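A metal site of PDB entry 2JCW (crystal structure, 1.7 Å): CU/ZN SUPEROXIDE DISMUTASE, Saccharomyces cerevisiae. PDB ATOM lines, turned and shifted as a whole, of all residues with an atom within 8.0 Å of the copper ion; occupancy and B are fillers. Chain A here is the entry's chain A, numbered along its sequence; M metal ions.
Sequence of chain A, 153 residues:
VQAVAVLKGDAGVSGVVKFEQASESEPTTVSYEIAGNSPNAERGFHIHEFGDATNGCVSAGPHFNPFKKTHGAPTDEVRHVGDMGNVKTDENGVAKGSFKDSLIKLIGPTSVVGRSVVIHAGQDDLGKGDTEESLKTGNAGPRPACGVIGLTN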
ATOM      1  N   GLY A  44     -20.646 -20.190 -20.826  1.00  0.00           N
ATOM      2  CA  GLY A  44     -20.277 -21.583 -21.059  1.00  0.00           C
ATOM      3  C   GLY A  44     -21.277 -22.535 -20.411  1.00  0.00           C
ATOM      4  O   GLY A  44     -21.619 -22.360 -19.255  1.00  0.00           O
ATOM      5  N   PHE A  45     -21.624 -23.599 -21.118  1.00  0.00           N
ATOM      6  CA  PHE A  45     -22.637 -24.571 -20.673  1.00  0.00           C
ATOM      7  C   PHE A  45     -22.144 -25.976 -21.064  1.00  0.00           C
ATOM      8  O   PHE A  45     -22.023 -26.277 -22.259  1.00  0.00           O
ATOM      9  CB  PHE A  45     -23.929 -24.196 -21.428  1.00  0.00           C
ATOM     10  CG  PHE A  45     -25.162 -24.929 -21.001  1.00  0.00           C
ATOM     11  CD1 PHE A  45     -25.483 -25.088 -19.647  1.00  0.00           C
ATOM     12  CD2 PHE A  45     -26.063 -25.391 -21.945  1.00  0.00           C
ATOM     13  CE1 PHE A  45     -26.678 -25.697 -19.254  1.00  0.00           C
ATOM     14  CE2 PHE A  45     -27.260 -25.996 -21.565  1.00  0.00           C
ATOM     15  CZ  PHE A  45     -27.569 -26.147 -20.211  1.00  0.00           C
ATOM     16  N   HIS A  46     -21.834 -26.835 -20.089  1.00  0.00           N
ATOM     17  CA  HIS A  46     -21.327 -28.169 -20.442  1.00  0.00           C
ATOM     18  C   HIS A  46     -21.755 -29.266 -19.492  1.00  0.00           C
ATOM     19  O   HIS A  46     -22.157 -29.010 -18.357  1.00  0.00           O
ATOM     20  CB  HIS A  46     -19.785 -28.219 -20.437  1.00  0.00           C
ATOM     21  CG  HIS A  46     -19.128 -26.939 -20.852  1.00  0.00           C
ATOM     22  ND1 HIS A  46     -18.479 -26.123 -19.958  1.00  0.00           N
ATOM     23  CD2 HIS A  46     -19.023 -26.349 -22.064  1.00  0.00           C
ATOM     24  CE1 HIS A  46     -17.999 -25.067 -20.609  1.00  0.00           C
ATOM     25  NE2 HIS A  46     -18.321 -25.187 -21.881  1.00  0.00           N
ATOM     26  N   ILE A  47     -21.565 -30.486 -19.961  1.00  0.00           N
ATOM     27  CA  ILE A  47     -21.809 -31.661 -19.152  1.00  0.00           C
ATOM     28  C   ILE A  47     -20.418 -32.101 -18.689  1.00  0.00           C
ATOM     29  O   ILE A  47     -19.483 -32.205 -19.483  1.00  0.00           O
ATOM     30  CB  ILE A  47     -22.514 -32.782 -19.923  1.00  0.00           C
ATOM     31  CG1 ILE A  47     -23.925 -32.297 -20.275  1.00  0.00           C
ATOM     32  CG2 ILE A  47     -22.587 -34.055 -19.058  1.00  0.00           C
ATOM     33  CD1 ILE A  47     -24.665 -33.207 -21.207  1.00  0.00           C
ATOM     34  N   HIS A  48     -20.245 -32.141 -17.374  1.00  0.00           N
ATOM     35  CA  HIS A  48     -19.001 -32.534 -16.755  1.00  0.00           C
ATOM     36  C   HIS A  48     -19.094 -34.001 -16.374  1.00  0.00           C
ATOM     37  O   HIS A  48     -20.203 -34.535 -16.168  1.00  0.00           O
ATOM     38  CB  HIS A  48     -18.707 -31.634 -15.556  1.00  0.00           C
ATOM     39  CG  HIS A  48     -18.247 -30.268 -15.938  1.00  0.00           C
ATOM     40  ND1 HIS A  48     -17.064 -29.727 -15.495  1.00  0.00           N
ATOM     41  CD2 HIS A  48     -18.803 -29.350 -16.759  1.00  0.00           C
ATOM     42  CE1 HIS A  48     -16.900 -28.529 -16.033  1.00  0.00           C
ATOM     43  NE2 HIS A  48     -17.938 -28.275 -16.797  1.00  0.00           N
ATOM     44  N   ALA A  60     -17.499 -31.858  -9.807  1.00  0.00           N
ATOM     45  CA  ALA A  60     -18.111 -32.327 -11.040  1.00  0.00           C
ATOM     46  C   ALA A  60     -16.995 -32.793 -11.989  1.00  0.00           C
ATOM     47  O   ALA A  60     -17.230 -33.507 -12.949  1.00  0.00           O
ATOM     48  CB  ALA A  60     -18.914 -31.193 -11.695  1.00  0.00           C
ATOM     49  N   GLY A  61     -15.771 -32.355 -11.735  1.00  0.00           N
ATOM     50  CA  GLY A  61     -14.666 -32.764 -12.586  1.00  0.00           C
ATOM     51  C   GLY A  61     -14.591 -32.010 -13.891  1.00  0.00           C
ATOM     52  O   GLY A  61     -15.175 -30.940 -14.031  1.00  0.00           O
ATOM     53  N   PRO A  62     -13.886 -32.568 -14.898  1.00  0.00           N
ATOM     54  CA  PRO A  62     -13.686 -31.996 -16.234  1.00  0.00           C
ATOM     55  C   PRO A  62     -14.872 -32.248 -17.164  1.00  0.00           C
ATOM     56  O   PRO A  62     -15.846 -32.902 -16.768  1.00  0.00           O
ATOM     57  CB  PRO A  62     -12.456 -32.744 -16.728  1.00  0.00           C
ATOM     58  CG  PRO A  62     -12.719 -34.128 -16.193  1.00  0.00           C
ATOM     59  CD  PRO A  62     -13.169 -33.860 -14.772  1.00  0.00           C
ATOM     60  N   HIS A  63     -14.815 -31.702 -18.372  1.00  0.00           N
ATOM     61  CA  HIS A  63     -15.889 -31.931 -19.337  1.00  0.00           C
ATOM     62  C   HIS A  63     -15.939 -33.419 -19.665  1.00  0.00           C
ATOM     63  O   HIS A  63     -14.902 -34.071 -19.775  1.00  0.00           O
ATOM     64  CB  HIS A  63     -15.640 -31.160 -20.623  1.00  0.00           C
ATOM     65  CG  HIS A  63     -15.623 -29.677 -20.439  1.00  0.00           C
ATOM     66  ND1 HIS A  63     -15.427 -28.795 -21.479  1.00  0.00           N
ATOM     67  CD2 HIS A  63     -15.757 -28.921 -19.323  1.00  0.00           C
ATOM     68  CE1 HIS A  63     -15.441 -27.562 -21.008  1.00  0.00           C
ATOM     69  NE2 HIS A  63     -15.645 -27.615 -19.705  1.00  0.00           N
ATOM     70  N   PHE A  64     -17.152 -33.938 -19.815  1.00  0.00           N
ATOM     71  CA  PHE A  64     -17.359 -35.336 -20.152  1.00  0.00           C
ATOM     72  C   PHE A  64     -16.704 -35.542 -21.524  1.00  0.00           C
ATOM     73  O   PHE A  64     -17.130 -34.935 -22.523  1.00  0.00           O
ATOM     74  CB  PHE A  64     -18.844 -35.665 -20.176  1.00  0.00           C
ATOM     75  CG  PHE A  64     -19.131 -37.122 -20.426  1.00  0.00           C
ATOM     76  CD1 PHE A  64     -18.395 -38.112 -19.773  1.00  0.00           C
ATOM     77  CD2 PHE A  64     -20.124 -37.503 -21.311  1.00  0.00           C
ATOM     78  CE1 PHE A  64     -18.646 -39.467 -20.002  1.00  0.00           C
ATOM     79  CE2 PHE A  64     -20.390 -38.862 -21.553  1.00  0.00           C
ATOM     80  CZ  PHE A  64     -19.647 -39.836 -20.897  1.00  0.00           C
ATOM     81  N   HIS A  71     -11.510 -29.692 -26.612  1.00  0.00           N
ATOM     82  CA  HIS A  71     -12.685 -28.864 -26.410  1.00  0.00           C
ATOM     83  C   HIS A  71     -13.063 -28.122 -27.692  1.00  0.00           C
ATOM     84  O   HIS A  71     -12.183 -27.627 -28.388  1.00  0.00           O
ATOM     85  CB  HIS A  71     -12.385 -27.855 -25.294  1.00  0.00           C
ATOM     86  CG  HIS A  71     -13.503 -26.904 -25.026  1.00  0.00           C
ATOM     87  ND1 HIS A  71     -14.603 -27.253 -24.262  1.00  0.00           N
ATOM     88  CD2 HIS A  71     -13.726 -25.652 -25.469  1.00  0.00           C
ATOM     89  CE1 HIS A  71     -15.450 -26.243 -24.254  1.00  0.00           C
ATOM     90  NE2 HIS A  71     -14.937 -25.265 -24.976  1.00  0.00           N
ATOM     91  N   GLY A  82     -19.527 -33.595 -23.831  1.00  0.00           N
ATOM     92  CA  GLY A  82     -20.226 -32.641 -22.981  1.00  0.00           C
ATOM     93  C   GLY A  82     -20.268 -31.172 -23.398  1.00  0.00           C
ATOM     94  O   GLY A  82     -20.890 -30.352 -22.723  1.00  0.00           O
ATOM     95  N   ASP A  83     -19.636 -30.843 -24.509  1.00  0.00           N
ATOM     96  CA  ASP A  83     -19.597 -29.462 -24.985  1.00  0.00           C
ATOM     97  C   ASP A  83     -20.927 -28.974 -25.572  1.00  0.00           C
ATOM     98  O   ASP A  83     -21.348 -29.399 -26.662  1.00  0.00           O
ATOM     99  CB  ASP A  83     -18.472 -29.273 -26.009  1.00  0.00           C
ATOM    100  CG  ASP A  83     -17.099 -29.369 -25.395  1.00  0.00           C
ATOM    101  OD1 ASP A  83     -16.922 -29.282 -24.151  1.00  0.00           O
ATOM    102  OD2 ASP A  83     -16.128 -29.541 -26.146  1.00  0.00           O
ATOM    103  N   MET A  84     -21.580 -28.064 -24.860  1.00  0.00           N
ATOM    104  CA  MET A  84     -22.854 -27.493 -25.308  1.00  0.00           C
ATOM    105  C   MET A  84     -22.725 -26.017 -25.686  1.00  0.00           C
ATOM    106  O   MET A  84     -23.720 -25.354 -25.935  1.00  0.00           O
ATOM    107  CB  MET A  84     -23.957 -27.717 -24.252  1.00  0.00           C
ATOM    108  CG  MET A  84     -24.210 -29.183 -23.984  1.00  0.00           C
ATOM    109  SD  MET A  84     -25.580 -29.462 -22.867  1.00  0.00           S
ATOM    110  CE  MET A  84     -24.873 -28.943 -21.305  1.00  0.00           C
ATOM    111  N   GLY A  85     -21.492 -25.530 -25.784  1.00  0.00           N
ATOM    112  CA  GLY A  85     -21.251 -24.150 -26.177  1.00  0.00           C
ATOM    113  C   GLY A  85     -21.642 -23.084 -25.165  1.00  0.00           C
ATOM    114  O   GLY A  85     -21.463 -23.266 -23.962  1.00  0.00           O
ATOM    115  N   SER A 116     -23.003 -34.397 -14.380  1.00  0.00           N
ATOM    116  CA  SER A 116     -23.443 -33.036 -14.017  1.00  0.00           C
ATOM    117  C   SER A 116     -23.524 -32.038 -15.143  1.00  0.00           C
ATOM    118  O   SER A 116     -22.764 -32.091 -16.108  1.00  0.00           O
ATOM    119  CB  SER A 116     -22.476 -32.403 -13.017  1.00  0.00           C
ATOM    120  OG  SER A 116     -22.490 -33.042 -11.752  1.00  0.00           O
ATOM    121  N   VAL A 117     -24.413 -31.065 -14.974  1.00  0.00           N
ATOM    122  CA  VAL A 117     -24.514 -29.968 -15.930  1.00  0.00           C
ATOM    123  C   VAL A 117     -23.937 -28.778 -15.163  1.00  0.00           C
ATOM    124  O   VAL A 117     -24.256 -28.574 -13.981  1.00  0.00           O
ATOM    125  CB  VAL A 117     -25.957 -29.617 -16.310  1.00  0.00           C
ATOM    126  CG1 VAL A 117     -25.942 -28.464 -17.286  1.00  0.00           C
ATOM    127  CG2 VAL A 117     -26.653 -30.817 -16.919  1.00  0.00           C
ATOM    128  N   VAL A 118     -23.059 -28.028 -15.813  1.00  0.00           N
ATOM    129  CA  VAL A 118     -22.428 -26.872 -15.198  1.00  0.00           C
ATOM    130  C   VAL A 118     -22.633 -25.637 -16.070  1.00  0.00           C
ATOM    131  O   VAL A 118     -22.463 -25.700 -17.286  1.00  0.00           O
ATOM    132  CB  VAL A 118     -20.905 -27.112 -14.980  1.00  0.00           C
ATOM    133  CG1 VAL A 118     -20.217 -25.837 -14.520  1.00  0.00           C
ATOM    134  CG2 VAL A 118     -20.686 -28.172 -13.953  1.00  0.00           C
ATOM    135  N   ILE A 119     -23.070 -24.542 -15.451  1.00  0.00           N
ATOM    136  CA  ILE A 119     -23.233 -23.267 -16.157  1.00  0.00           C
ATOM    137  C   ILE A 119     -22.067 -22.422 -15.625  1.00  0.00           C
ATOM    138  O   ILE A 119     -21.789 -22.403 -14.423  1.00  0.00           O
ATOM    139  CB  ILE A 119     -24.634 -22.571 -15.884  1.00  0.00           C
ATOM    140  CG1 ILE A 119     -24.743 -21.209 -16.599  1.00  0.00           C
ATOM    141  CG2 ILE A 119     -24.873 -22.357 -14.388  1.00  0.00           C
ATOM    142  CD1 ILE A 119     -24.872 -21.253 -18.114  1.00  0.00           C
ATOM    143  N   HIS A 120     -21.333 -21.792 -16.534  1.00  0.00           N
ATOM    144  CA  HIS A 120     -20.178 -20.984 -16.157  1.00  0.00           C
ATOM    145  C   HIS A 120     -20.431 -19.496 -16.015  1.00  0.00           C
ATOM    146  O   HIS A 120     -21.443 -18.979 -16.470  1.00  0.00           O
ATOM    147  CB  HIS A 120     -19.039 -21.210 -17.144  1.00  0.00           C
ATOM    148  CG  HIS A 120     -18.437 -22.572 -17.025  1.00  0.00           C
ATOM    149  ND1 HIS A 120     -17.360 -22.833 -16.210  1.00  0.00           N
ATOM    150  CD2 HIS A 120     -18.799 -23.755 -17.575  1.00  0.00           C
ATOM    151  CE1 HIS A 120     -17.080 -24.125 -16.262  1.00  0.00           C
ATOM    152  NE2 HIS A 120     -17.943 -24.711 -17.074  1.00  0.00           N
ATOM    153  N   ASP A 124     -17.437 -19.213 -23.178  1.00  0.00           N
ATOM    154  CA  ASP A 124     -16.659 -20.328 -23.691  1.00  0.00           C
ATOM    155  C   ASP A 124     -16.044 -19.841 -25.024  1.00  0.00           C
ATOM    156  O   ASP A 124     -16.769 -19.370 -25.903  1.00  0.00           O
ATOM    157  CB  ASP A 124     -17.626 -21.495 -23.918  1.00  0.00           C
ATOM    158  CG  ASP A 124     -16.935 -22.789 -24.300  1.00  0.00           C
ATOM    159  OD1 ASP A 124     -15.809 -22.770 -24.828  1.00  0.00           O
ATOM    160  OD2 ASP A 124     -17.561 -23.844 -24.105  1.00  0.00           O
ATOM    161  N   LYS A 136      -9.022 -27.275 -23.451  1.00  0.00           N
ATOM    162  CA  LYS A 136      -9.446 -28.115 -22.346  1.00  0.00           C
ATOM    163  C   LYS A 136     -10.774 -27.661 -21.764  1.00  0.00           C
ATOM    164  O   LYS A 136     -11.709 -28.455 -21.633  1.00  0.00           O
ATOM    165  CB  LYS A 136      -8.401 -28.127 -21.217  1.00  0.00           C
ATOM    166  CG  LYS A 136      -6.958 -28.247 -21.665  1.00  0.00           C
ATOM    167  CD  LYS A 136      -6.674 -29.577 -22.349  1.00  0.00           C
ATOM    168  CE  LYS A 136      -5.238 -29.647 -22.909  1.00  0.00           C
ATOM    169  NZ  LYS A 136      -4.993 -28.725 -24.073  1.00  0.00           N
ATOM    170  N   THR A 137     -10.874 -26.373 -21.455  1.00  0.00           N
ATOM    171  CA  THR A 137     -12.088 -25.834 -20.841  1.00  0.00           C
ATOM    172  C   THR A 137     -12.793 -24.736 -21.634  1.00  0.00           C
ATOM    173  O   THR A 137     -13.928 -24.363 -21.306  1.00  0.00           O
ATOM    174  CB  THR A 137     -11.780 -25.256 -19.454  1.00  0.00           C
ATOM    175  OG1 THR A 137     -10.964 -24.092 -19.616  1.00  0.00           O
ATOM    176  CG2 THR A 137     -11.014 -26.253 -18.593  1.00  0.00           C
ATOM    177  N   GLY A 138     -12.136 -24.222 -22.664  1.00  0.00           N
ATOM    178  CA  GLY A 138     -12.725 -23.135 -23.428  1.00  0.00           C
ATOM    179  C   GLY A 138     -12.602 -21.824 -22.663  1.00  0.00           C
ATOM    180  O   GLY A 138     -13.236 -20.835 -23.037  1.00  0.00           O
ATOM    181  N   ALA A 140     -13.887 -20.938 -19.983  1.00  0.00           N
ATOM    182  CA  ALA A 140     -15.203 -20.491 -19.530  1.00  0.00           C
ATOM    183  C   ALA A 140     -15.269 -19.932 -18.099  1.00  0.00           C
ATOM    184  O   ALA A 140     -16.282 -19.355 -17.709  1.00  0.00           O
ATOM    185  CB  ALA A 140     -16.216 -21.612 -19.724  1.00  0.00           C
ATOM    186  N   GLY A 141     -14.221 -20.136 -17.317  1.00  0.00           N
ATOM    187  CA  GLY A 141     -14.181 -19.586 -15.981  1.00  0.00           C
ATOM    188  C   GLY A 141     -14.866 -20.345 -14.876  1.00  0.00           C
ATOM    189  O   GLY A 141     -15.082 -21.557 -14.992  1.00  0.00           O
ATOM    190  N   PRO A 142     -15.224 -19.659 -13.785  1.00  0.00           N
ATOM    191  CA  PRO A 142     -15.902 -20.232 -12.596  1.00  0.00           C
ATOM    192  C   PRO A 142     -17.235 -20.945 -12.902  1.00  0.00           C
ATOM    193  O   PRO A 142     -17.865 -20.727 -13.938  1.00  0.00           O
ATOM    194  CB  PRO A 142     -16.094 -19.019 -11.676  1.00  0.00           C
ATOM    195  CG  PRO A 142     -14.991 -18.069 -12.106  1.00  0.00           C
ATOM    196  CD  PRO A 142     -14.962 -18.216 -13.609  1.00  0.00           C
ATOM    197  N   ARG A 143     -17.677 -21.757 -11.935  1.00  0.00           N
ATOM    198  CA  ARG A 143     -18.905 -22.555 -12.030  1.00  0.00           C
ATOM    199  C   ARG A 143     -19.906 -22.097 -10.962  1.00  0.00           C
ATOM    200  O   ARG A 143     -19.963 -22.684  -9.875  1.00  0.00           O
ATOM    201  CB  ARG A 143     -18.571 -24.020 -11.758  1.00  0.00           C
ATOM    202  CG  ARG A 143     -17.390 -24.547 -12.563  1.00  0.00           C
ATOM    203  CD  ARG A 143     -17.024 -25.959 -12.179  1.00  0.00           C
ATOM    204  NE  ARG A 143     -15.854 -26.390 -12.928  1.00  0.00           N
ATOM    205  CZ  ARG A 143     -15.388 -27.631 -12.969  1.00  0.00           C
ATOM    206  NH1 ARG A 143     -15.971 -28.605 -12.279  1.00  0.00           N
ATOM    207  NH2 ARG A 143     -14.346 -27.900 -13.735  1.00  0.00           N
ATOM    208  N   ALA A 145     -23.154 -22.411 -10.807  1.00  0.00           N
ATOM    209  CA  ALA A 145     -24.224 -23.348 -10.521  1.00  0.00           C
ATOM    210  C   ALA A 145     -24.028 -24.657 -11.280  1.00  0.00           C
ATOM    211  O   ALA A 145     -23.359 -24.699 -12.331  1.00  0.00           O
ATOM    212  CB  ALA A 145     -25.587 -22.726 -10.859  1.00  0.00           C
HETATM  213 CU    CU M   1     -18.088 -26.591 -17.984  1.00  0.00          CU
HETATM  214 ZN    ZN M   2     -15.221 -29.196 -23.434  1.00  0.00          ZN
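NE2 of His 63 touches the copper ion, 3.2 Å away. Of the 29 residues printed, 4 come within 4 Å of the copper ion. The nearest printed residue that does not touch the copper ion is Val 118 (4.1 Å).
The copper ion is bound by ND1 of His 46 (2.1 Å), NE2 of His 48 (2.1 Å) and NE2 of His 120 (2.1 Å). The copper ion has three donor atoms within binding distance.
A ring nitrogen (ND1) of His 46 lies close to a ring nitrogen (NE2) of His 63 (3.2 Å). N of Val 118 is in hydrogen-bond range of O of His 46. O of Gly 44 is in hydrogen-bond range of N of His 120 (2.8 Å). The side-chain carboxylate of Asp 124 is in hydrogen-bond range of a ring nitrogen (NE2) of His 46. A ring nitrogen (ND1) of His 120 sits at hydrogen-bond distance from the backbone carbonyl oxygen of Pro 142 (3.1 Å). The backbone NH (N) of His 48 sits at hydrogen-bond distance from the backbone carbonyl oxygen (O) of Ser 116, at 2.8 Å. A ring nitrogen (ND1) of His 48 lies within hydrogen-bond range of the backbone carbonyl oxygen (O) of Gly 61, at 2.7 Å. O of Gly 141 lies within hydrogen-bond range of ND1 of His 120.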
